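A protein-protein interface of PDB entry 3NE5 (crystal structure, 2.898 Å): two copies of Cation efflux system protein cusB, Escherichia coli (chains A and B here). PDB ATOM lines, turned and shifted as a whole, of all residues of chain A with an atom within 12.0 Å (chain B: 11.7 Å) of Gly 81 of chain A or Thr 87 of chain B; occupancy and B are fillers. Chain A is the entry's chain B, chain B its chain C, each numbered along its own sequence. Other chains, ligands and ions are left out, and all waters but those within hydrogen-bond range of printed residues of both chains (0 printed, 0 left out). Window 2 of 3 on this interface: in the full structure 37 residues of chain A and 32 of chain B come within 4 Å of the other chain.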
ATOM      1  N   ALA A  79      -0.387 -25.100  11.910  1.00  0.00           N
ATOM      2  CA  ALA A  79       0.018 -24.146  12.936  1.00  0.00           C
ATOM      3  C   ALA A  79       0.149 -24.825  14.295  1.00  0.00           C
ATOM      4  O   ALA A  79      -0.365 -24.330  15.298  1.00  0.00           O
ATOM      5  CB  ALA A  79      -0.973 -22.995  13.010  1.00  0.00           C
ATOM      6  N   SER A  80       0.843 -25.959  14.321  1.00  0.00           N
ATOM      7  CA  SER A  80       1.026 -26.716  15.554  1.00  0.00           C
ATOM      8  C   SER A  80       1.961 -26.003  16.526  1.00  0.00           C
ATOM      9  O   SER A  80       3.080 -25.635  16.169  1.00  0.00           O
ATOM     10  CB  SER A  80       1.563 -28.116  15.252  1.00  0.00           C
ATOM     11  OG  SER A  80       0.602 -28.896  14.562  1.00  0.00           O
ATOM     12  N   GLY A  81       1.492 -25.813  17.755  1.00  0.00           N
ATOM     13  CA  GLY A  81       2.315 -25.241  18.805  1.00  0.00           C
ATOM     14  C   GLY A  81       3.063 -26.330  19.550  1.00  0.00           C
ATOM     15  O   GLY A  81       3.495 -26.138  20.687  1.00  0.00           O
ATOM     16  N   VAL A  82       3.213 -27.479  18.898  1.00  0.00           N
ATOM     17  CA  VAL A  82       3.893 -28.625  19.489  1.00  0.00           C
ATOM     18  C   VAL A  82       5.373 -28.331  19.712  1.00  0.00           C
ATOM     19  O   VAL A  82       6.119 -28.084  18.765  1.00  0.00           O
ATOM     20  CB  VAL A  82       3.734 -29.883  18.610  1.00  0.00           C
ATOM     21  CG1 VAL A  82       4.211 -29.606  17.190  1.00  0.00           C
ATOM     22  CG2 VAL A  82       4.480 -31.061  19.218  1.00  0.00           C
ATOM     23  N   ARG A  83       5.791 -28.356  20.973  1.00  0.00           N
ATOM     24  CA  ARG A  83       7.159 -28.004  21.330  1.00  0.00           C
ATOM     25  C   ARG A  83       8.042 -29.226  21.534  1.00  0.00           C
ATOM     26  O   ARG A  83       7.571 -30.299  21.912  1.00  0.00           O
ATOM     27  CB  ARG A  83       7.181 -27.137  22.590  1.00  0.00           C
ATOM     28  CG  ARG A  83       6.745 -25.702  22.365  1.00  0.00           C
ATOM     29  CD  ARG A  83       7.680 -24.993  21.400  1.00  0.00           C
ATOM     30  NE  ARG A  83       9.083 -25.250  21.713  1.00  0.00           N
ATOM     31  CZ  ARG A  83       9.766 -24.620  22.664  1.00  0.00           C
ATOM     32  NH1 ARG A  83       9.175 -23.692  23.404  1.00  0.00           N
ATOM     33  NH2 ARG A  83      11.040 -24.921  22.876  1.00  0.00           N
ATOM     34  N   ILE A  84       9.333 -29.048  21.284  1.00  0.00           N
ATOM     35  CA  ILE A  84      10.303 -30.116  21.447  1.00  0.00           C
ATOM     36  C   ILE A  84      11.553 -29.575  22.125  1.00  0.00           C
ATOM     37  O   ILE A  84      11.867 -28.390  22.011  1.00  0.00           O
ATOM     38  CB  ILE A  84      10.683 -30.716  20.085  1.00  0.00           C
ATOM     39  CG1 ILE A  84      11.991 -31.495  20.178  1.00  0.00           C
ATOM     40  CG2 ILE A  84      10.833 -29.620  19.056  1.00  0.00           C
ATOM     41  CD1 ILE A  84      12.751 -31.537  18.871  1.00  0.00           C
ATOM     42  N   ASP A  85      12.255 -30.442  22.845  1.00  0.00           N
ATOM     43  CA  ASP A  85      13.525 -30.073  23.449  1.00  0.00           C
ATOM     44  C   ASP A  85      14.626 -30.092  22.395  1.00  0.00           C
ATOM     45  O   ASP A  85      14.997 -31.154  21.897  1.00  0.00           O
ATOM     46  CB  ASP A  85      13.875 -31.033  24.581  1.00  0.00           C
ATOM     47  CG  ASP A  85      15.233 -30.751  25.175  1.00  0.00           C
ATOM     48  OD1 ASP A  85      15.641 -29.571  25.181  1.00  0.00           O
ATOM     49  OD2 ASP A  85      15.891 -31.706  25.635  1.00  0.00           O
ATOM     50  N   PRO A  86      15.156 -28.908  22.056  1.00  0.00           N
ATOM     51  CA  PRO A  86      16.153 -28.737  20.992  1.00  0.00           C
ATOM     52  C   PRO A  86      17.539 -29.265  21.362  1.00  0.00           C
ATOM     53  O   PRO A  86      18.239 -29.784  20.493  1.00  0.00           O
ATOM     54  CB  PRO A  86      16.211 -27.213  20.799  1.00  0.00           C
ATOM     55  CG  PRO A  86      15.065 -26.651  21.591  1.00  0.00           C
ATOM     56  CD  PRO A  86      14.803 -27.627  22.683  1.00  0.00           C
ATOM     57  N   THR A  87      17.926 -29.132  22.626  1.00  0.00           N
ATOM     58  CA  THR A  87      19.247 -29.574  23.071  1.00  0.00           C
ATOM     59  C   THR A  87      19.478 -31.042  22.725  1.00  0.00           C
ATOM     60  O   THR A  87      18.544 -31.840  22.744  1.00  0.00           O
ATOM     61  CB  THR A  87      19.424 -29.395  24.590  1.00  0.00           C
ATOM     62  OG1 THR A  87      18.749 -30.453  25.281  1.00  0.00           O
ATOM     63  CG2 THR A  87      18.860 -28.058  25.039  1.00  0.00           C
ATOM     64  N   ARG B  83       9.639 -13.432   8.355  1.00  0.00           N
ATOM     65  CA  ARG B  83       8.940 -13.865   9.560  1.00  0.00           C
ATOM     66  C   ARG B  83       8.970 -15.386   9.659  1.00  0.00           C
ATOM     67  O   ARG B  83       8.900 -16.080   8.645  1.00  0.00           O
ATOM     68  CB  ARG B  83       7.492 -13.366   9.540  1.00  0.00           C
ATOM     69  CG  ARG B  83       6.809 -13.332  10.902  1.00  0.00           C
ATOM     70  CD  ARG B  83       5.352 -12.888  10.784  1.00  0.00           C
ATOM     71  NE  ARG B  83       5.181 -11.798   9.825  1.00  0.00           N
ATOM     72  CZ  ARG B  83       4.562 -11.918   8.654  1.00  0.00           C
ATOM     73  NH1 ARG B  83       4.041 -13.083   8.293  1.00  0.00           N
ATOM     74  NH2 ARG B  83       4.457 -10.871   7.844  1.00  0.00           N
ATOM     75  N   ILE B  84       9.083 -15.901  10.879  1.00  0.00           N
ATOM     76  CA  ILE B  84       9.131 -17.342  11.097  1.00  0.00           C
ATOM     77  C   ILE B  84       8.388 -17.735  12.369  1.00  0.00           C
ATOM     78  O   ILE B  84       8.539 -17.099  13.412  1.00  0.00           O
ATOM     79  CB  ILE B  84      10.580 -17.859  11.185  1.00  0.00           C
ATOM     80  CG1 ILE B  84      11.368 -17.475   9.932  1.00  0.00           C
ATOM     81  CG2 ILE B  84      10.597 -19.366  11.381  1.00  0.00           C
ATOM     82  CD1 ILE B  84      12.832 -17.848  10.000  1.00  0.00           C
ATOM     83  N   ASP B  85       7.587 -18.792  12.272  1.00  0.00           N
ATOM     84  CA  ASP B  85       6.793 -19.270  13.396  1.00  0.00           C
ATOM     85  C   ASP B  85       7.671 -19.503  14.622  1.00  0.00           C
ATOM     86  O   ASP B  85       8.602 -20.307  14.582  1.00  0.00           O
ATOM     87  CB  ASP B  85       6.058 -20.557  13.011  1.00  0.00           C
ATOM     88  CG  ASP B  85       4.927 -20.891  13.962  1.00  0.00           C
ATOM     89  OD1 ASP B  85       4.119 -21.785  13.633  1.00  0.00           O
ATOM     90  OD2 ASP B  85       4.840 -20.260  15.035  1.00  0.00           O
ATOM     91  N   PRO B  86       7.375 -18.789  15.718  1.00  0.00           N
ATOM     92  CA  PRO B  86       8.139 -18.860  16.968  1.00  0.00           C
ATOM     93  C   PRO B  86       8.294 -20.283  17.499  1.00  0.00           C
ATOM     94  O   PRO B  86       9.263 -20.566  18.201  1.00  0.00           O
ATOM     95  CB  PRO B  86       7.299 -18.024  17.937  1.00  0.00           C
ATOM     96  CG  PRO B  86       6.606 -17.041  17.061  1.00  0.00           C
ATOM     97  CD  PRO B  86       6.297 -17.786  15.789  1.00  0.00           C
ATOM     98  N   THR B  87       7.354 -21.162  17.172  1.00  0.00           N
ATOM     99  CA  THR B  87       7.448 -22.548  17.611  1.00  0.00           C
ATOM    100  C   THR B  87       8.541 -23.282  16.843  1.00  0.00           C
ATOM    101  O   THR B  87       9.274 -24.089  17.412  1.00  0.00           O
ATOM    102  CB  THR B  87       6.108 -23.290  17.459  1.00  0.00           C
ATOM    103  OG1 THR B  87       5.613 -23.117  16.127  1.00  0.00           O
ATOM    104  CG2 THR B  87       5.088 -22.749  18.448  1.00  0.00           C
ATOM    105  N   GLN B  88       8.655 -22.994  15.551  1.00  0.00           N
ATOM    106  CA  GLN B  88       9.698 -23.604  14.736  1.00  0.00           C
ATOM    107  C   GLN B  88      11.086 -23.162  15.193  1.00  0.00           C
ATOM    108  O   GLN B  88      11.997 -23.980  15.300  1.00  0.00           O
ATOM    109  CB  GLN B  88       9.495 -23.277  13.258  1.00  0.00           C
ATOM    110  CG  GLN B  88       8.329 -24.005  12.625  1.00  0.00           C
ATOM    111  CD  GLN B  88       8.077 -23.562  11.202  1.00  0.00           C
ATOM    112  OE1 GLN B  88       8.941 -22.958  10.565  1.00  0.00           O
ATOM    113  NE2 GLN B  88       6.889 -23.859  10.693  1.00  0.00           N
ATOM    114  N   THR B  89      11.243 -21.869  15.462  1.00  0.00           N
ATOM    115  CA  THR B  89      12.524 -21.348  15.928  1.00  0.00           C
ATOM    116  C   THR B  89      12.862 -21.892  17.309  1.00  0.00           C
ATOM    117  O   THR B  89      14.015 -22.215  17.590  1.00  0.00           O
ATOM    118  CB  THR B  89      12.549 -19.811  15.969  1.00  0.00           C
ATOM    119  OG1 THR B  89      11.505 -19.333  16.824  1.00  0.00           O
ATOM    120  CG2 THR B  89      12.367 -19.239  14.574  1.00  0.00           C
ATOM    121  N   GLN B  90      11.860 -21.990  18.173  1.00  0.00           N
ATOM    122  CA  GLN B  90      12.067 -22.562  19.496  1.00  0.00           C
ATOM    123  C   GLN B  90      12.508 -24.012  19.373  1.00  0.00           C
ATOM    124  O   GLN B  90      13.386 -24.467  20.102  1.00  0.00           O
ATOM    125  CB  GLN B  90      10.790 -22.468  20.329  1.00  0.00           C
ATOM    126  CG  GLN B  90      10.497 -21.080  20.850  1.00  0.00           C
ATOM    127  CD  GLN B  90       9.122 -20.986  21.463  1.00  0.00           C
ATOM    128  OE1 GLN B  90       8.311 -21.902  21.334  1.00  0.00           O
ATOM    129  NE2 GLN B  90       8.846 -19.875  22.134  1.00  0.00           N
ATOM    130  N   ASN B  91      11.894 -24.734  18.444  1.00  0.00           N
ATOM    131  CA  ASN B  91      12.273 -26.114  18.177  1.00  0.00           C
ATOM    132  C   ASN B  91      13.684 -26.194  17.607  1.00  0.00           C
ATOM    133  O   ASN B  91      14.454 -27.093  17.949  1.00  0.00           O
ATOM    134  CB  ASN B  91      11.283 -26.759  17.204  1.00  0.00           C
ATOM    135  CG  ASN B  91       9.898 -26.920  17.801  1.00  0.00           C
ATOM    136  OD1 ASN B  91       9.707 -26.761  19.007  1.00  0.00           O
ATOM    137  ND2 ASN B  91       8.924 -27.245  16.957  1.00  0.00           N
ATOM    138  N   LEU B  92      14.012 -25.246  16.736  1.00  0.00           N
ATOM    139  CA  LEU B  92      15.325 -25.187  16.108  1.00  0.00           C
ATOM    140  C   LEU B  92      16.400 -24.915  17.152  1.00  0.00           C
ATOM    141  O   LEU B  92      17.576 -25.201  16.937  1.00  0.00           O
ATOM    142  CB  LEU B  92      15.351 -24.087  15.044  1.00  0.00           C
ATOM    143  CG  LEU B  92      16.667 -23.857  14.297  1.00  0.00           C
ATOM    144  CD1 LEU B  92      17.154 -25.150  13.664  1.00  0.00           C
ATOM    145  CD2 LEU B  92      16.505 -22.769  13.245  1.00  0.00           C
ATOM    146  N   GLY B  93      15.989 -24.357  18.284  1.00  0.00           N
ATOM    147  CA  GLY B  93      16.930 -23.967  19.315  1.00  0.00           C
ATOM    148  C   GLY B  93      17.748 -22.745  18.936  1.00  0.00           C
ATOM    149  O   GLY B  93      18.948 -22.683  19.211  1.00  0.00           O
ATOM    150  N   VAL B  94      17.096 -21.768  18.310  1.00  0.00           N
ATOM    151  CA  VAL B  94      17.760 -20.532  17.903  1.00  0.00           C
ATOM    152  C   VAL B  94      18.422 -19.831  19.095  1.00  0.00           C
ATOM    153  O   VAL B  94      17.819 -19.698  20.159  1.00  0.00           O
ATOM    154  CB  VAL B  94      16.775 -19.573  17.179  1.00  0.00           C
ATOM    155  CG1 VAL B  94      17.278 -18.139  17.195  1.00  0.00           C
ATOM    156  CG2 VAL B  94      16.534 -20.034  15.739  1.00  0.00           C
ATOM    157  N   LYS B  95      19.677 -19.420  18.920  1.00  0.00           N
ATOM    158  CA  LYS B  95      20.354 -18.592  19.914  1.00  0.00           C
ATOM    159  C   LYS B  95      20.779 -17.258  19.299  1.00  0.00           C
ATOM    160  O   LYS B  95      21.030 -17.166  18.089  1.00  0.00           O
ATOM    161  CB  LYS B  95      21.526 -19.320  20.565  1.00  0.00           C
ATOM    162  CG  LYS B  95      21.110 -20.466  21.490  1.00  0.00           C
ATOM    163  CD  LYS B  95      22.233 -21.482  21.689  1.00  0.00           C
ATOM    164  CE  LYS B  95      21.810 -22.623  22.618  1.00  0.00           C
ATOM    165  NZ  LYS B  95      22.668 -23.837  22.478  1.00  0.00           N
ATOM    166  N   ASP B 347      10.336  -7.033  16.400  1.00  0.00           N
ATOM    167  CA  ASP B 347       9.164  -7.890  16.269  1.00  0.00           C
ATOM    168  C   ASP B 347       9.529  -9.368  16.354  1.00  0.00           C
ATOM    169  O   ASP B 347       8.657 -10.225  16.492  1.00  0.00           O
ATOM    170  CB  ASP B 347       8.462  -7.613  14.939  1.00  0.00           C
ATOM    171  CG  ASP B 347       8.171  -6.143  14.731  1.00  0.00           C
ATOM    172  OD1 ASP B 347       7.641  -5.505  15.664  1.00  0.00           O
ATOM    173  OD2 ASP B 347       8.472  -5.625  13.634  1.00  0.00           O
ATOM    174  N   GLY B 348      10.821  -9.662  16.269  1.00  0.00           N
ATOM    175  CA  GLY B 348      11.288 -11.034  16.228  1.00  0.00           C
ATOM    176  C   GLY B 348      11.577 -11.432  14.795  1.00  0.00           C
ATOM    177  O   GLY B 348      12.066 -12.529  14.522  1.00  0.00           O
ATOM    178  N   PHE B 350      13.371 -11.859  11.386  1.00  0.00           N
ATOM    179  CA  PHE B 350      14.776 -12.098  11.071  1.00  0.00           C
ATOM    180  C   PHE B 350      15.190 -11.376   9.795  1.00  0.00           C
ATOM    181  O   PHE B 350      14.834 -11.789   8.694  1.00  0.00           O
ATOM    182  CB  PHE B 350      15.046 -13.596  10.944  1.00  0.00           C
ATOM    183  CG  PHE B 350      14.746 -14.369  12.194  1.00  0.00           C
ATOM    184  CD1 PHE B 350      15.744 -14.628  13.119  1.00  0.00           C
ATOM    185  CD2 PHE B 350      13.465 -14.828  12.450  1.00  0.00           C
ATOM    186  CE1 PHE B 350      15.469 -15.335  14.272  1.00  0.00           C
ATOM    187  CE2 PHE B 350      13.184 -15.537  13.601  1.00  0.00           C
ATOM    188  CZ  PHE B 350      14.188 -15.791  14.514  1.00  0.00           C
ATOM    189  N   LEU B 384      19.891 -22.608   8.786  1.00  0.00           N
ATOM    190  CA  LEU B 384      18.514 -22.813   8.352  1.00  0.00           C
ATOM    191  C   LEU B 384      17.753 -21.498   8.236  1.00  0.00           C
ATOM    192  O   LEU B 384      17.033 -21.270   7.266  1.00  0.00           O
ATOM    193  CB  LEU B 384      17.782 -23.760   9.302  1.00  0.00           C
ATOM    194  CG  LEU B 384      18.148 -25.235   9.164  1.00  0.00           C
ATOM    195  CD1 LEU B 384      17.213 -26.087  10.005  1.00  0.00           C
ATOM    196  CD2 LEU B 384      18.096 -25.657   7.705  1.00  0.00           C
ATOM    197  N   ILE B 385      17.918 -20.636   9.233  1.00  0.00           N
ATOM    198  CA  ILE B 385      17.247 -19.344   9.235  1.00  0.00           C
ATOM    199  C   ILE B 385      17.695 -18.485   8.061  1.00  0.00           C
ATOM    200  O   ILE B 385      16.886 -17.798   7.437  1.00  0.00           O
ATOM    201  CB  ILE B 385      17.508 -18.580  10.534  1.00  0.00           C
ATOM    202  CG1 ILE B 385      16.809 -19.270  11.702  1.00  0.00           C
ATOM    203  CG2 ILE B 385      17.019 -17.153  10.407  1.00  0.00           C
ATOM    204  CD1 ILE B 385      16.677 -18.392  12.914  1.00  0.00           C
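OG1 of Thr 87 of chain B touches O of Ser 80 of chain A (3.6 Å).
CA of Gly 81 of chain A touches CG2 of Thr 87 of chain B (3.7 Å).
O of Gln 90 of chain B touches CG of Pro 86 of chain A, 3.1 Å away.
Asn 91 of chain B touches Pro 86 of chain A (O to CB, 3.4 Å).
CB of Pro 86 of chain A touches CA of Gly 93 of chain B, at 3.6 Å.
No residue of chain B comes within 4 Å of Ala 79 of chain A.
Ser 80 of chain A touches one residue of chain B.
Printed residues of chain B within 4 Å of Val 82 of chain A: Asn 91 (3.4 Å).
Arg 83 of chain A touches just these residues of chain B: Gln 90 and Asn 91.
Of the printed residues of chain B, Ile 84 of chain A touches Asn 91.
Of the printed residues of chain B, Pro 86 of chain A touches Gln 90 (3.1 Å), Asn 91 (3.4 Å) and Gly 93 (3.6 Å).
Ile 84 of chain B touches none of the printed residues of chain A.
Pro 86 of chain B touches none of the printed residues of chain A.
Thr 87 of chain B touches just these residues of chain A: Ser 80 and Gly 81.
Gln 88 of chain B touches none of the printed residues of chain A.
No residue of chain A comes within 4 Å of Thr 89 of chain B.
Gly 348 of chain B touches none of the printed residues of chain A.
The nearest residue of chain A that does not touch Thr 87 of chain B is Arg 83 of chain A (4.4 Å).
The nearest printed residue of chain B that does not touch Ile 84 of chain A is Gln 90 of chain B (4.6 Å).
Printed residues of chain B that touch a printed residue of chain A: Thr 87, Gln 90, Asn 91 and Gly 93.
Of the 9 printed residues of chain A, 6 touch a printed residue of chain B.
Printed residues of chain A that touch a printed residue of chain B: Ser 80, Gly 81, Val 82, Arg 83, Ile 84 and Pro 86.
Hydrophobic or aromatic side chains of chain A within 4 Å of the printed part of chain B: Ile 84 and Pro 86.
Among the printed residues, 9 pairs touch across the chains.
Among the printed residues, no Asp or Glu carboxylate lies within 4 Å of a Lys or Arg side-chain nitrogen of the other chain.
The backbone carbonyl oxygen (O) of Val 82 of chain A lies within hydrogen-bond range of the side-chain amide nitrogen (ND2) of Asn 91 of chain B (3.4 Å).
The side-chain amide oxygen of Gln 90 of chain B lies within hydrogen-bond range of the guanidinium group of Arg 83 of chain A (2.9 Å).
The side-chain amide oxygen (OD1) of Asn 91 of chain B lies within hydrogen-bond range of the guanidinium group (NE) of Arg 83 of chain A (3.2 Å).
OD1 of Asn 91 of chain B sits close to N of Ile 84 of chain A (3.2 Å).
5 positions are printed for both chains.
The side-chain hydroxyl of Thr 87 of chain B sits at hydrogen-bond distance from the side-chain carboxylate of Asp 85 of chain B, at 3.2 Å.
The backbone carbonyl oxygen (O) of Thr 87 of chain B sits close to the side-chain amide oxygen (OD1) of Asn 91 of chain B (3.1 Å).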
